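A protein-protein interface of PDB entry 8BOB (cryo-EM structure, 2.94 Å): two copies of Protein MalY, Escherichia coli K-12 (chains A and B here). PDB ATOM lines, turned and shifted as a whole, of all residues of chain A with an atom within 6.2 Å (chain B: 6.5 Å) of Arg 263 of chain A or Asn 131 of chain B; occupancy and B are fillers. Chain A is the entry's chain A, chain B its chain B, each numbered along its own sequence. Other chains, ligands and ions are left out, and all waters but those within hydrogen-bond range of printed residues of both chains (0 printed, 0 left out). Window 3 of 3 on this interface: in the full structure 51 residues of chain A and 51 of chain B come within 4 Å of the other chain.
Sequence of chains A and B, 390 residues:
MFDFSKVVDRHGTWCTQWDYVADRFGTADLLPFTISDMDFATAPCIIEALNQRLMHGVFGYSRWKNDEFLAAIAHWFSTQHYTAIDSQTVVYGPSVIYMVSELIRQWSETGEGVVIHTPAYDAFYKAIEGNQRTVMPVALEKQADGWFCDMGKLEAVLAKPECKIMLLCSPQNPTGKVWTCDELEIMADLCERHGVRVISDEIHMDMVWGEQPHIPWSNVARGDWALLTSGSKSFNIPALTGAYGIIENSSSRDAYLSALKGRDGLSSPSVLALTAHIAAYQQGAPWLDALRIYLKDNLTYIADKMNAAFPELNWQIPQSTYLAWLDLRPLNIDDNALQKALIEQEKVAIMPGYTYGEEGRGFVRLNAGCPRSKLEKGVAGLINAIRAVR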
ATOM      1  N   TYR A  98      -1.309  -9.197  13.659  1.00  0.00           N
ATOM      2  CA  TYR A  98      -2.698  -9.468  13.993  1.00  0.00           C
ATOM      3  C   TYR A  98      -3.549  -8.225  13.811  1.00  0.00           C
ATOM      4  O   TYR A  98      -4.649  -8.293  13.252  1.00  0.00           O
ATOM      5  CB  TYR A  98      -2.833  -9.982  15.419  1.00  0.00           C
ATOM      6  CG  TYR A  98      -4.280 -10.101  15.801  1.00  0.00           C
ATOM      7  CD1 TYR A  98      -5.072 -11.088  15.257  1.00  0.00           C
ATOM      8  CD2 TYR A  98      -4.868  -9.200  16.663  1.00  0.00           C
ATOM      9  CE1 TYR A  98      -6.394 -11.195  15.578  1.00  0.00           C
ATOM     10  CE2 TYR A  98      -6.196  -9.298  16.989  1.00  0.00           C
ATOM     11  CZ  TYR A  98      -6.953 -10.297  16.442  1.00  0.00           C
ATOM     12  OH  TYR A  98      -8.280 -10.406  16.760  1.00  0.00           O
ATOM     13  N   GLU A 102      -6.671  -7.702  11.282  1.00  0.00           N
ATOM     14  CA  GLU A 102      -7.992  -7.320  11.756  1.00  0.00           C
ATOM     15  C   GLU A 102      -8.479  -6.068  11.046  1.00  0.00           C
ATOM     16  O   GLU A 102      -9.631  -6.003  10.598  1.00  0.00           O
ATOM     17  CB  GLU A 102      -7.964  -7.118  13.264  1.00  0.00           C
ATOM     18  CG  GLU A 102      -9.242  -6.555  13.824  1.00  0.00           C
ATOM     19  CD  GLU A 102     -10.481  -7.274  13.326  1.00  0.00           C
ATOM     20  OE1 GLU A 102     -10.500  -8.518  13.336  1.00  0.00           O
ATOM     21  OE2 GLU A 102     -11.445  -6.592  12.925  1.00  0.00           O
ATOM     22  N   ARG A 105      -9.548  -6.939   7.582  1.00  0.00           N
ATOM     23  CA  ARG A 105     -10.872  -7.541   7.603  1.00  0.00           C
ATOM     24  C   ARG A 105     -11.952  -6.507   7.849  1.00  0.00           C
ATOM     25  O   ARG A 105     -13.108  -6.725   7.477  1.00  0.00           O
ATOM     26  CB  ARG A 105     -10.947  -8.620   8.676  1.00  0.00           C
ATOM     27  CG  ARG A 105     -10.363  -9.944   8.259  1.00  0.00           C
ATOM     28  CD  ARG A 105     -10.717 -11.029   9.245  1.00  0.00           C
ATOM     29  NE  ARG A 105     -10.162 -10.774  10.565  1.00  0.00           N
ATOM     30  CZ  ARG A 105      -8.933 -11.106  10.928  1.00  0.00           C
ATOM     31  NH1 ARG A 105      -8.129 -11.699  10.067  1.00  0.00           N
ATOM     32  NH2 ARG A 105      -8.506 -10.844  12.148  1.00  0.00           N
ATOM     33  N   SER A 258     -14.056  -4.510  19.933  1.00  0.00           N
ATOM     34  CA  SER A 258     -15.069  -5.551  20.019  1.00  0.00           C
ATOM     35  C   SER A 258     -14.564  -6.849  19.415  1.00  0.00           C
ATOM     36  O   SER A 258     -14.736  -7.923  19.996  1.00  0.00           O
ATOM     37  CB  SER A 258     -16.344  -5.096  19.320  1.00  0.00           C
ATOM     38  OG  SER A 258     -17.312  -6.122  19.328  1.00  0.00           O
ATOM     39  N   ALA A 259     -13.934  -6.769  18.245  1.00  0.00           N
ATOM     40  CA  ALA A 259     -13.415  -7.982  17.625  1.00  0.00           C
ATOM     41  C   ALA A 259     -12.310  -8.605  18.465  1.00  0.00           C
ATOM     42  O   ALA A 259     -12.185  -9.828  18.532  1.00  0.00           O
ATOM     43  CB  ALA A 259     -12.912  -7.682  16.219  1.00  0.00           C
ATOM     44  N   LEU A 260     -11.501  -7.781  19.115  1.00  0.00           N
ATOM     45  CA  LEU A 260     -10.376  -8.315  19.866  1.00  0.00           C
ATOM     46  C   LEU A 260     -10.844  -8.994  21.140  1.00  0.00           C
ATOM     47  O   LEU A 260     -10.354 -10.068  21.498  1.00  0.00           O
ATOM     48  CB  LEU A 260      -9.384  -7.205  20.192  1.00  0.00           C
ATOM     49  CG  LEU A 260      -8.294  -7.590  21.184  1.00  0.00           C
ATOM     50  CD1 LEU A 260      -7.142  -8.225  20.472  1.00  0.00           C
ATOM     51  CD2 LEU A 260      -7.833  -6.383  21.944  1.00  0.00           C
ATOM     52  N   LYS A 261     -11.786  -8.383  21.845  1.00  0.00           N
ATOM     53  CA  LYS A 261     -12.216  -8.953  23.113  1.00  0.00           C
ATOM     54  C   LYS A 261     -13.322  -9.979  22.922  1.00  0.00           C
ATOM     55  O   LYS A 261     -13.265 -11.070  23.487  1.00  0.00           O
ATOM     56  CB  LYS A 261     -12.676  -7.844  24.057  1.00  0.00           C
ATOM     57  CG  LYS A 261     -12.949  -8.298  25.473  1.00  0.00           C
ATOM     58  CD  LYS A 261     -14.415  -8.520  25.706  1.00  0.00           C
ATOM     59  CE  LYS A 261     -15.168  -7.214  25.660  1.00  0.00           C
ATOM     60  NZ  LYS A 261     -16.638  -7.433  25.728  1.00  0.00           N
ATOM     61  N   GLY A 262     -14.327  -9.649  22.130  1.00  0.00           N
ATOM     62  CA  GLY A 262     -15.468 -10.524  21.998  1.00  0.00           C
ATOM     63  C   GLY A 262     -15.250 -11.706  21.084  1.00  0.00           C
ATOM     64  O   GLY A 262     -15.296 -12.854  21.525  1.00  0.00           O
ATOM     65  N   ARG A 263     -14.998 -11.439  19.807  1.00  0.00           N
ATOM     66  CA  ARG A 263     -15.012 -12.507  18.819  1.00  0.00           C
ATOM     67  C   ARG A 263     -13.818 -13.438  18.965  1.00  0.00           C
ATOM     68  O   ARG A 263     -13.955 -14.651  18.795  1.00  0.00           O
ATOM     69  CB  ARG A 263     -15.048 -11.918  17.420  1.00  0.00           C
ATOM     70  CG  ARG A 263     -15.205 -12.943  16.349  1.00  0.00           C
ATOM     71  CD  ARG A 263     -14.738 -12.392  15.041  1.00  0.00           C
ATOM     72  NE  ARG A 263     -13.321 -12.087  15.096  1.00  0.00           N
ATOM     73  CZ  ARG A 263     -12.712 -11.255  14.268  1.00  0.00           C
ATOM     74  NH1 ARG A 263     -13.406 -10.643  13.325  1.00  0.00           N
ATOM     75  NH2 ARG A 263     -11.415 -11.033  14.387  1.00  0.00           N
ATOM     76  N   ASP A 264     -12.636 -12.903  19.262  1.00  0.00           N
ATOM     77  CA  ASP A 264     -11.430 -13.715  19.287  1.00  0.00           C
ATOM     78  C   ASP A 264     -10.858 -13.938  20.675  1.00  0.00           C
ATOM     79  O   ASP A 264      -9.859 -14.644  20.795  1.00  0.00           O
ATOM     80  CB  ASP A 264     -10.343 -13.089  18.409  1.00  0.00           C
ATOM     81  CG  ASP A 264     -10.727 -13.049  16.954  1.00  0.00           C
ATOM     82  OD1 ASP A 264     -11.793 -13.587  16.606  1.00  0.00           O
ATOM     83  OD2 ASP A 264      -9.966 -12.472  16.153  1.00  0.00           O
ATOM     84  N   GLY A 265     -11.438 -13.351  21.713  1.00  0.00           N
ATOM     85  CA  GLY A 265     -10.993 -13.617  23.070  1.00  0.00           C
ATOM     86  C   GLY A 265      -9.516 -13.421  23.327  1.00  0.00           C
ATOM     87  O   GLY A 265      -8.903 -14.225  24.034  1.00  0.00           O
ATOM     88  N   ILE B  97     -10.154 -19.450  23.953  1.00  0.00           N
ATOM     89  CA  ILE B  97     -11.288 -18.922  23.211  1.00  0.00           C
ATOM     90  C   ILE B  97     -10.885 -18.569  21.793  1.00  0.00           C
ATOM     91  O   ILE B  97     -11.696 -18.674  20.868  1.00  0.00           O
ATOM     92  CB  ILE B  97     -11.895 -17.722  23.946  1.00  0.00           C
ATOM     93  CG1 ILE B  97     -12.404 -18.166  25.304  1.00  0.00           C
ATOM     94  CG2 ILE B  97     -13.045 -17.168  23.161  1.00  0.00           C
ATOM     95  CD1 ILE B  97     -13.524 -19.158  25.210  1.00  0.00           C
ATOM     96  N   TYR B  98      -9.633 -18.165  21.582  1.00  0.00           N
ATOM     97  CA  TYR B  98      -9.194 -17.915  20.219  1.00  0.00           C
ATOM     98  C   TYR B  98      -9.278 -19.180  19.385  1.00  0.00           C
ATOM     99  O   TYR B  98      -9.747 -19.150  18.244  1.00  0.00           O
ATOM    100  CB  TYR B  98      -7.773 -17.370  20.187  1.00  0.00           C
ATOM    101  CG  TYR B  98      -7.279 -17.273  18.773  1.00  0.00           C
ATOM    102  CD1 TYR B  98      -7.779 -16.317  17.916  1.00  0.00           C
ATOM    103  CD2 TYR B  98      -6.352 -18.165  18.279  1.00  0.00           C
ATOM    104  CE1 TYR B  98      -7.355 -16.231  16.623  1.00  0.00           C
ATOM    105  CE2 TYR B  98      -5.921 -18.088  16.979  1.00  0.00           C
ATOM    106  CZ  TYR B  98      -6.428 -17.119  16.158  1.00  0.00           C
ATOM    107  OH  TYR B  98      -6.005 -17.032  14.858  1.00  0.00           O
ATOM    108  N   VAL B 100     -11.186 -21.782  19.970  1.00  0.00           N
ATOM    109  CA  VAL B 100     -12.603 -22.075  19.780  1.00  0.00           C
ATOM    110  C   VAL B 100     -13.151 -21.287  18.603  1.00  0.00           C
ATOM    111  O   VAL B 100     -13.839 -21.828  17.734  1.00  0.00           O
ATOM    112  CB  VAL B 100     -13.391 -21.773  21.063  1.00  0.00           C
ATOM    113  CG1 VAL B 100     -14.861 -21.752  20.771  1.00  0.00           C
ATOM    114  CG2 VAL B 100     -13.084 -22.792  22.112  1.00  0.00           C
ATOM    115  N   SER B 101     -12.844 -19.995  18.554  1.00  0.00           N
ATOM    116  CA  SER B 101     -13.388 -19.145  17.503  1.00  0.00           C
ATOM    117  C   SER B 101     -12.819 -19.509  16.142  1.00  0.00           C
ATOM    118  O   SER B 101     -13.538 -19.495  15.138  1.00  0.00           O
ATOM    119  CB  SER B 101     -13.106 -17.689  17.828  1.00  0.00           C
ATOM    120  OG  SER B 101     -11.715 -17.470  17.870  1.00  0.00           O
ATOM    121  N   GLU B 102     -11.533 -19.834  16.084  1.00  0.00           N
ATOM    122  CA  GLU B 102     -10.945 -20.233  14.816  1.00  0.00           C
ATOM    123  C   GLU B 102     -11.584 -21.513  14.301  1.00  0.00           C
ATOM    124  O   GLU B 102     -11.935 -21.614  13.120  1.00  0.00           O
ATOM    125  CB  GLU B 102      -9.439 -20.398  14.969  1.00  0.00           C
ATOM    126  CG  GLU B 102      -8.765 -20.974  13.754  1.00  0.00           C
ATOM    127  CD  GLU B 102      -9.178 -20.295  12.462  1.00  0.00           C
ATOM    128  OE1 GLU B 102      -9.195 -19.052  12.413  1.00  0.00           O
ATOM    129  OE2 GLU B 102      -9.483 -21.007  11.486  1.00  0.00           O
ATOM    130  N   ILE B 104     -14.564 -22.571  15.009  1.00  0.00           N
ATOM    131  CA  ILE B 104     -15.925 -22.263  14.588  1.00  0.00           C
ATOM    132  C   ILE B 104     -15.920 -21.645  13.202  1.00  0.00           C
ATOM    133  O   ILE B 104     -16.768 -21.961  12.363  1.00  0.00           O
ATOM    134  CB  ILE B 104     -16.613 -21.339  15.601  1.00  0.00           C
ATOM    135  CG1 ILE B 104     -16.886 -22.079  16.898  1.00  0.00           C
ATOM    136  CG2 ILE B 104     -17.904 -20.824  15.038  1.00  0.00           C
ATOM    137  CD1 ILE B 104     -17.168 -21.165  18.046  1.00  0.00           C
ATOM    138  N   ARG B 105     -14.969 -20.751  12.938  1.00  0.00           N
ATOM    139  CA  ARG B 105     -14.854 -20.178  11.605  1.00  0.00           C
ATOM    140  C   ARG B 105     -14.497 -21.229  10.574  1.00  0.00           C
ATOM    141  O   ARG B 105     -14.780 -21.045   9.387  1.00  0.00           O
ATOM    142  CB  ARG B 105     -13.804 -19.075  11.592  1.00  0.00           C
ATOM    143  CG  ARG B 105     -14.296 -17.749  12.107  1.00  0.00           C
ATOM    144  CD  ARG B 105     -13.311 -16.647  11.809  1.00  0.00           C
ATOM    145  NE  ARG B 105     -12.035 -16.858  12.474  1.00  0.00           N
ATOM    146  CZ  ARG B 105     -11.780 -16.490  13.721  1.00  0.00           C
ATOM    147  NH1 ARG B 105     -12.716 -15.902  14.437  1.00  0.00           N
ATOM    148  NH2 ARG B 105     -10.592 -16.713  14.250  1.00  0.00           N
ATOM    149  N   GLU B 109     -20.327 -22.452   8.435  1.00  0.00           N
ATOM    150  CA  GLU B 109     -20.489 -21.207   7.709  1.00  0.00           C
ATOM    151  C   GLU B 109     -21.141 -20.163   8.604  1.00  0.00           C
ATOM    152  O   GLU B 109     -21.327 -20.362   9.804  1.00  0.00           O
ATOM    153  CB  GLU B 109     -21.319 -21.417   6.448  1.00  0.00           C
ATOM    154  CG  GLU B 109     -21.025 -22.696   5.718  1.00  0.00           C
ATOM    155  CD  GLU B 109     -19.571 -22.836   5.372  1.00  0.00           C
ATOM    156  OE1 GLU B 109     -18.987 -21.857   4.868  1.00  0.00           O
ATOM    157  OE2 GLU B 109     -19.009 -23.924   5.606  1.00  0.00           O
ATOM    158  N   THR B 110     -21.495 -19.030   8.012  1.00  0.00           N
ATOM    159  CA  THR B 110     -22.237 -18.005   8.725  1.00  0.00           C
ATOM    160  C   THR B 110     -23.709 -18.381   8.768  1.00  0.00           C
ATOM    161  O   THR B 110     -24.270 -18.830   7.768  1.00  0.00           O
ATOM    162  CB  THR B 110     -22.059 -16.652   8.049  1.00  0.00           C
ATOM    163  OG1 THR B 110     -22.229 -16.807   6.638  1.00  0.00           O
ATOM    164  CG2 THR B 110     -20.683 -16.103   8.322  1.00  0.00           C
ATOM    165  N   GLY B 111     -24.326 -18.215   9.927  1.00  0.00           N
ATOM    166  CA  GLY B 111     -25.732 -18.502  10.085  1.00  0.00           C
ATOM    167  C   GLY B 111     -26.048 -19.903  10.551  1.00  0.00           C
ATOM    168  O   GLY B 111     -27.219 -20.199  10.807  1.00  0.00           O
ATOM    169  N   LYS B 126     -20.134 -14.798  23.225  1.00  0.00           N
ATOM    170  CA  LYS B 126     -19.383 -13.795  22.484  1.00  0.00           C
ATOM    171  C   LYS B 126     -18.689 -14.414  21.285  1.00  0.00           C
ATOM    172  O   LYS B 126     -18.787 -13.905  20.168  1.00  0.00           O
ATOM    173  CB  LYS B 126     -18.365 -13.128  23.401  1.00  0.00           C
ATOM    174  CG  LYS B 126     -18.980 -12.413  24.577  1.00  0.00           C
ATOM    175  CD  LYS B 126     -19.815 -11.251  24.113  1.00  0.00           C
ATOM    176  CE  LYS B 126     -20.932 -10.961  25.088  1.00  0.00           C
ATOM    177  NZ  LYS B 126     -22.031 -11.953  24.972  1.00  0.00           N
ATOM    178  N   ALA B 127     -17.993 -15.527  21.496  1.00  0.00           N
ATOM    179  CA  ALA B 127     -17.260 -16.156  20.407  1.00  0.00           C
ATOM    180  C   ALA B 127     -18.200 -16.684  19.336  1.00  0.00           C
ATOM    181  O   ALA B 127     -17.877 -16.635  18.145  1.00  0.00           O
ATOM    182  CB  ALA B 127     -16.384 -17.280  20.947  1.00  0.00           C
ATOM    183  N   ILE B 128     -19.366 -17.184  19.728  1.00  0.00           N
ATOM    184  CA  ILE B 128     -20.252 -17.796  18.751  1.00  0.00           C
ATOM    185  C   ILE B 128     -20.973 -16.743  17.935  1.00  0.00           C
ATOM    186  O   ILE B 128     -21.073 -16.858  16.711  1.00  0.00           O
ATOM    187  CB  ILE B 128     -21.238 -18.739  19.448  1.00  0.00           C
ATOM    188  CG1 ILE B 128     -20.496 -19.941  20.008  1.00  0.00           C
ATOM    189  CG2 ILE B 128     -22.272 -19.210  18.481  1.00  0.00           C
ATOM    190  CD1 ILE B 128     -21.301 -20.731  20.982  1.00  0.00           C
ATOM    191  N   GLU B 129     -21.490 -15.701  18.581  1.00  0.00           N
ATOM    192  CA  GLU B 129     -22.256 -14.707  17.843  1.00  0.00           C
ATOM    193  C   GLU B 129     -21.365 -13.669  17.179  1.00  0.00           C
ATOM    194  O   GLU B 129     -21.747 -13.105  16.152  1.00  0.00           O
ATOM    195  CB  GLU B 129     -23.262 -14.034  18.766  1.00  0.00           C
ATOM    196  CG  GLU B 129     -24.490 -14.877  19.010  1.00  0.00           C
ATOM    197  CD  GLU B 129     -25.071 -14.671  20.389  1.00  0.00           C
ATOM    198  OE1 GLU B 129     -24.338 -14.186  21.276  1.00  0.00           O
ATOM    199  OE2 GLU B 129     -26.260 -14.994  20.584  1.00  0.00           O
ATOM    200  N   GLY B 130     -20.182 -13.413  17.736  1.00  0.00           N
ATOM    201  CA  GLY B 130     -19.241 -12.532  17.078  1.00  0.00           C
ATOM    202  C   GLY B 130     -18.889 -12.991  15.683  1.00  0.00           C
ATOM    203  O   GLY B 130     -18.616 -12.170  14.807  1.00  0.00           O
ATOM    204  N   ASN B 131     -18.896 -14.295  15.451  1.00  0.00           N
ATOM    205  CA  ASN B 131     -18.697 -14.844  14.124  1.00  0.00           C
ATOM    206  C   ASN B 131     -19.996 -14.993  13.361  1.00  0.00           C
ATOM    207  O   ASN B 131     -19.992 -15.568  12.273  1.00  0.00           O
ATOM    208  CB  ASN B 131     -17.999 -16.196  14.210  1.00  0.00           C
ATOM    209  CG  ASN B 131     -16.670 -16.110  14.894  1.00  0.00           C
ATOM    210  OD1 ASN B 131     -15.671 -15.761  14.281  1.00  0.00           O
ATOM    211  ND2 ASN B 131     -16.646 -16.424  16.174  1.00  0.00           N
ATOM    212  N   GLN B 132     -21.102 -14.497  13.909  1.00  0.00           N
ATOM    213  CA  GLN B 132     -22.410 -14.589  13.272  1.00  0.00           C
ATOM    214  C   GLN B 132     -22.815 -16.042  13.054  1.00  0.00           C
ATOM    215  O   GLN B 132     -23.246 -16.443  11.972  1.00  0.00           O
ATOM    216  CB  GLN B 132     -22.444 -13.809  11.961  1.00  0.00           C
ATOM    217  CG  GLN B 132     -22.198 -12.338  12.139  1.00  0.00           C
ATOM    218  CD  GLN B 132     -20.805 -11.949  11.735  1.00  0.00           C
ATOM    219  OE1 GLN B 132     -20.317 -12.366  10.689  1.00  0.00           O
ATOM    220  NE2 GLN B 132     -20.148 -11.153  12.564  1.00  0.00           N
ATOM    221  N   ARG B 133     -22.663 -16.836  14.100  1.00  0.00           N
ATOM    222  CA  ARG B 133     -23.184 -18.190  14.154  1.00  0.00           C
ATOM    223  C   ARG B 133     -24.206 -18.244  15.276  1.00  0.00           C
ATOM    224  O   ARG B 133     -23.963 -17.707  16.359  1.00  0.00           O
ATOM    225  CB  ARG B 133     -22.063 -19.197  14.395  1.00  0.00           C
ATOM    226  CG  ARG B 133     -21.483 -19.781  13.134  1.00  0.00           C
ATOM    227  CD  ARG B 133     -20.439 -18.880  12.539  1.00  0.00           C
ATOM    228  NE  ARG B 133     -19.769 -19.515  11.413  1.00  0.00           N
ATOM    229  CZ  ARG B 133     -18.810 -18.945  10.699  1.00  0.00           C
ATOM    230  NH1 ARG B 133     -18.408 -17.720  10.985  1.00  0.00           N
ATOM    231  NH2 ARG B 133     -18.255 -19.599   9.695  1.00  0.00           N
ATOM    232  N   ASP B 264      -3.217 -14.569  10.659  1.00  0.00           N
ATOM    233  CA  ASP B 264      -3.308 -13.731  11.843  1.00  0.00           C
ATOM    234  C   ASP B 264      -1.977 -13.462  12.520  1.00  0.00           C
ATOM    235  O   ASP B 264      -1.955 -12.731  13.508  1.00  0.00           O
ATOM    236  CB  ASP B 264      -4.256 -14.355  12.871  1.00  0.00           C
ATOM    237  CG  ASP B 264      -5.675 -14.439  12.372  1.00  0.00           C
ATOM    238  OD1 ASP B 264      -5.946 -13.934  11.269  1.00  0.00           O
ATOM    239  OD2 ASP B 264      -6.521 -15.019  13.079  1.00  0.00           O
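NH1 of Arg 105 of chain A lies within salt-bridge range of OD1 of Asp 264 of chain B (3.3 Å).
The side-chain carboxylate (OD1) of Asp 264 of chain A lies within salt-bridge range of the guanidinium group (NH1) of Arg 105 of chain B, at 3.3 Å.
The side-chain carboxylate (OE1) of Glu 102 of chain B lies within salt-bridge range of the guanidinium group (NH2) of Arg 105 of chain B (3.3 Å).
The side-chain amide oxygen (OD1) of Asn 131 of chain B lies within hydrogen-bond range of the guanidinium group (NH1) of Arg 105 of chain B (3.0 Å).
O of Ile 97 of chain B lies within hydrogen-bond range of OG of Ser 101 of chain B, 3.2 Å away.
The side-chain hydroxyl (OH) of Tyr 98 of chain A lies within hydrogen-bond range of the side-chain carboxylate (OD2) of Asp 264 of chain A, 2.7 Å away.
The side-chain carboxylate (OD1) of Asp 264 of chain A is in salt-bridge range of the guanidinium group (NE) of Arg 263 of chain A, 2.6 Å away.
The backbone carbonyl oxygen of Gly 130 of chain B lies within hydrogen-bond range of the side-chain amide nitrogen of Gln 132 of chain B.
CA of Tyr 98 of chain A touches O of Asp 264 of chain B, 3.4 Å away.
O of Gly 262 of chain A touches CB of Lys 126 of chain B, 3.6 Å away.
Gly 262 of chain A touches Ala 127 of chain B (O to N, 3.8 Å).
Arg 263 of chain A touches Ser 101 of chain B (O to CB, 3.3 Å).
Arg 105 of chain B touches Arg 263 of chain A.
O of Arg 263 of chain A touches CA of Ala 127 of chain B, at 3.97 Å.
Gly 130 of chain B touches Arg 263 of chain A.
CG of Arg 263 of chain A touches OD1 of Asn 131 of chain B (3.5 Å).
Tyr 98 of chain B touches Asp 264 of chain A (CA to O, 3.4 Å).
Of the printed residues of chain B, Tyr 98 of chain A touches Asp 264 (3.4 Å).
Ala 259 of chain A touches none of the printed residues of chain B.
Of chain B, only Ser 101 (3.3 Å), Arg 105 (3.9 Å), Ala 127 (3.97 Å), Gly 130 (3.7 Å) and Asn 131 (3.5 Å) come within 4 Å of Arg 263 of chain A.
Of the printed residues of chain A, Ser 101 of chain B touches Arg 263 (3.3 Å).
Printed residues of chain A within 4 Å of Lys 126 of chain B: Gly 262.
Asn 131 of chain B touches just one residue of chain A: Arg 263.
The nearest residue of chain A that does not touch Asn 131 of chain B is Asp 264 of chain A (5.0 Å).
Printed residues of chain B that touch a printed residue of chain A: Tyr 98, Ser 101, Arg 105, Lys 126, Ala 127, Gly 130, Asn 131 and Asp 264.
Hydrophobic or aromatic side chains of chain B within 4 Å of the printed part of chain A: Tyr 98.
Of the 11 printed residues of chain A, 5 touch a printed residue of chain B.
Among the printed residues, 11 pairs touch across the chains.
Among the printed residues, Asp or Glu carboxylates within 4 Å of a Lys or Arg side-chain nitrogen of the other chain: Arg 105 of chain A with Asp 264 of chain B (3.3 Å) and Asp 264 of chain A with Arg 105 of chain B (3.3 Å).
Tyr 98 of chain A touches Asp 264 of chain B, and with the chains exchanged Asp 264 of chain A touches Tyr 98 of chain B.
Arg 105 of chain A touches Asp 264 of chain B, and with the chains exchanged Asp 264 of chain A touches Arg 105 of chain B.
Of the 11 pairs that touch across the chains among the printed residues, 4 have their exchanged pair printed and touching as well.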
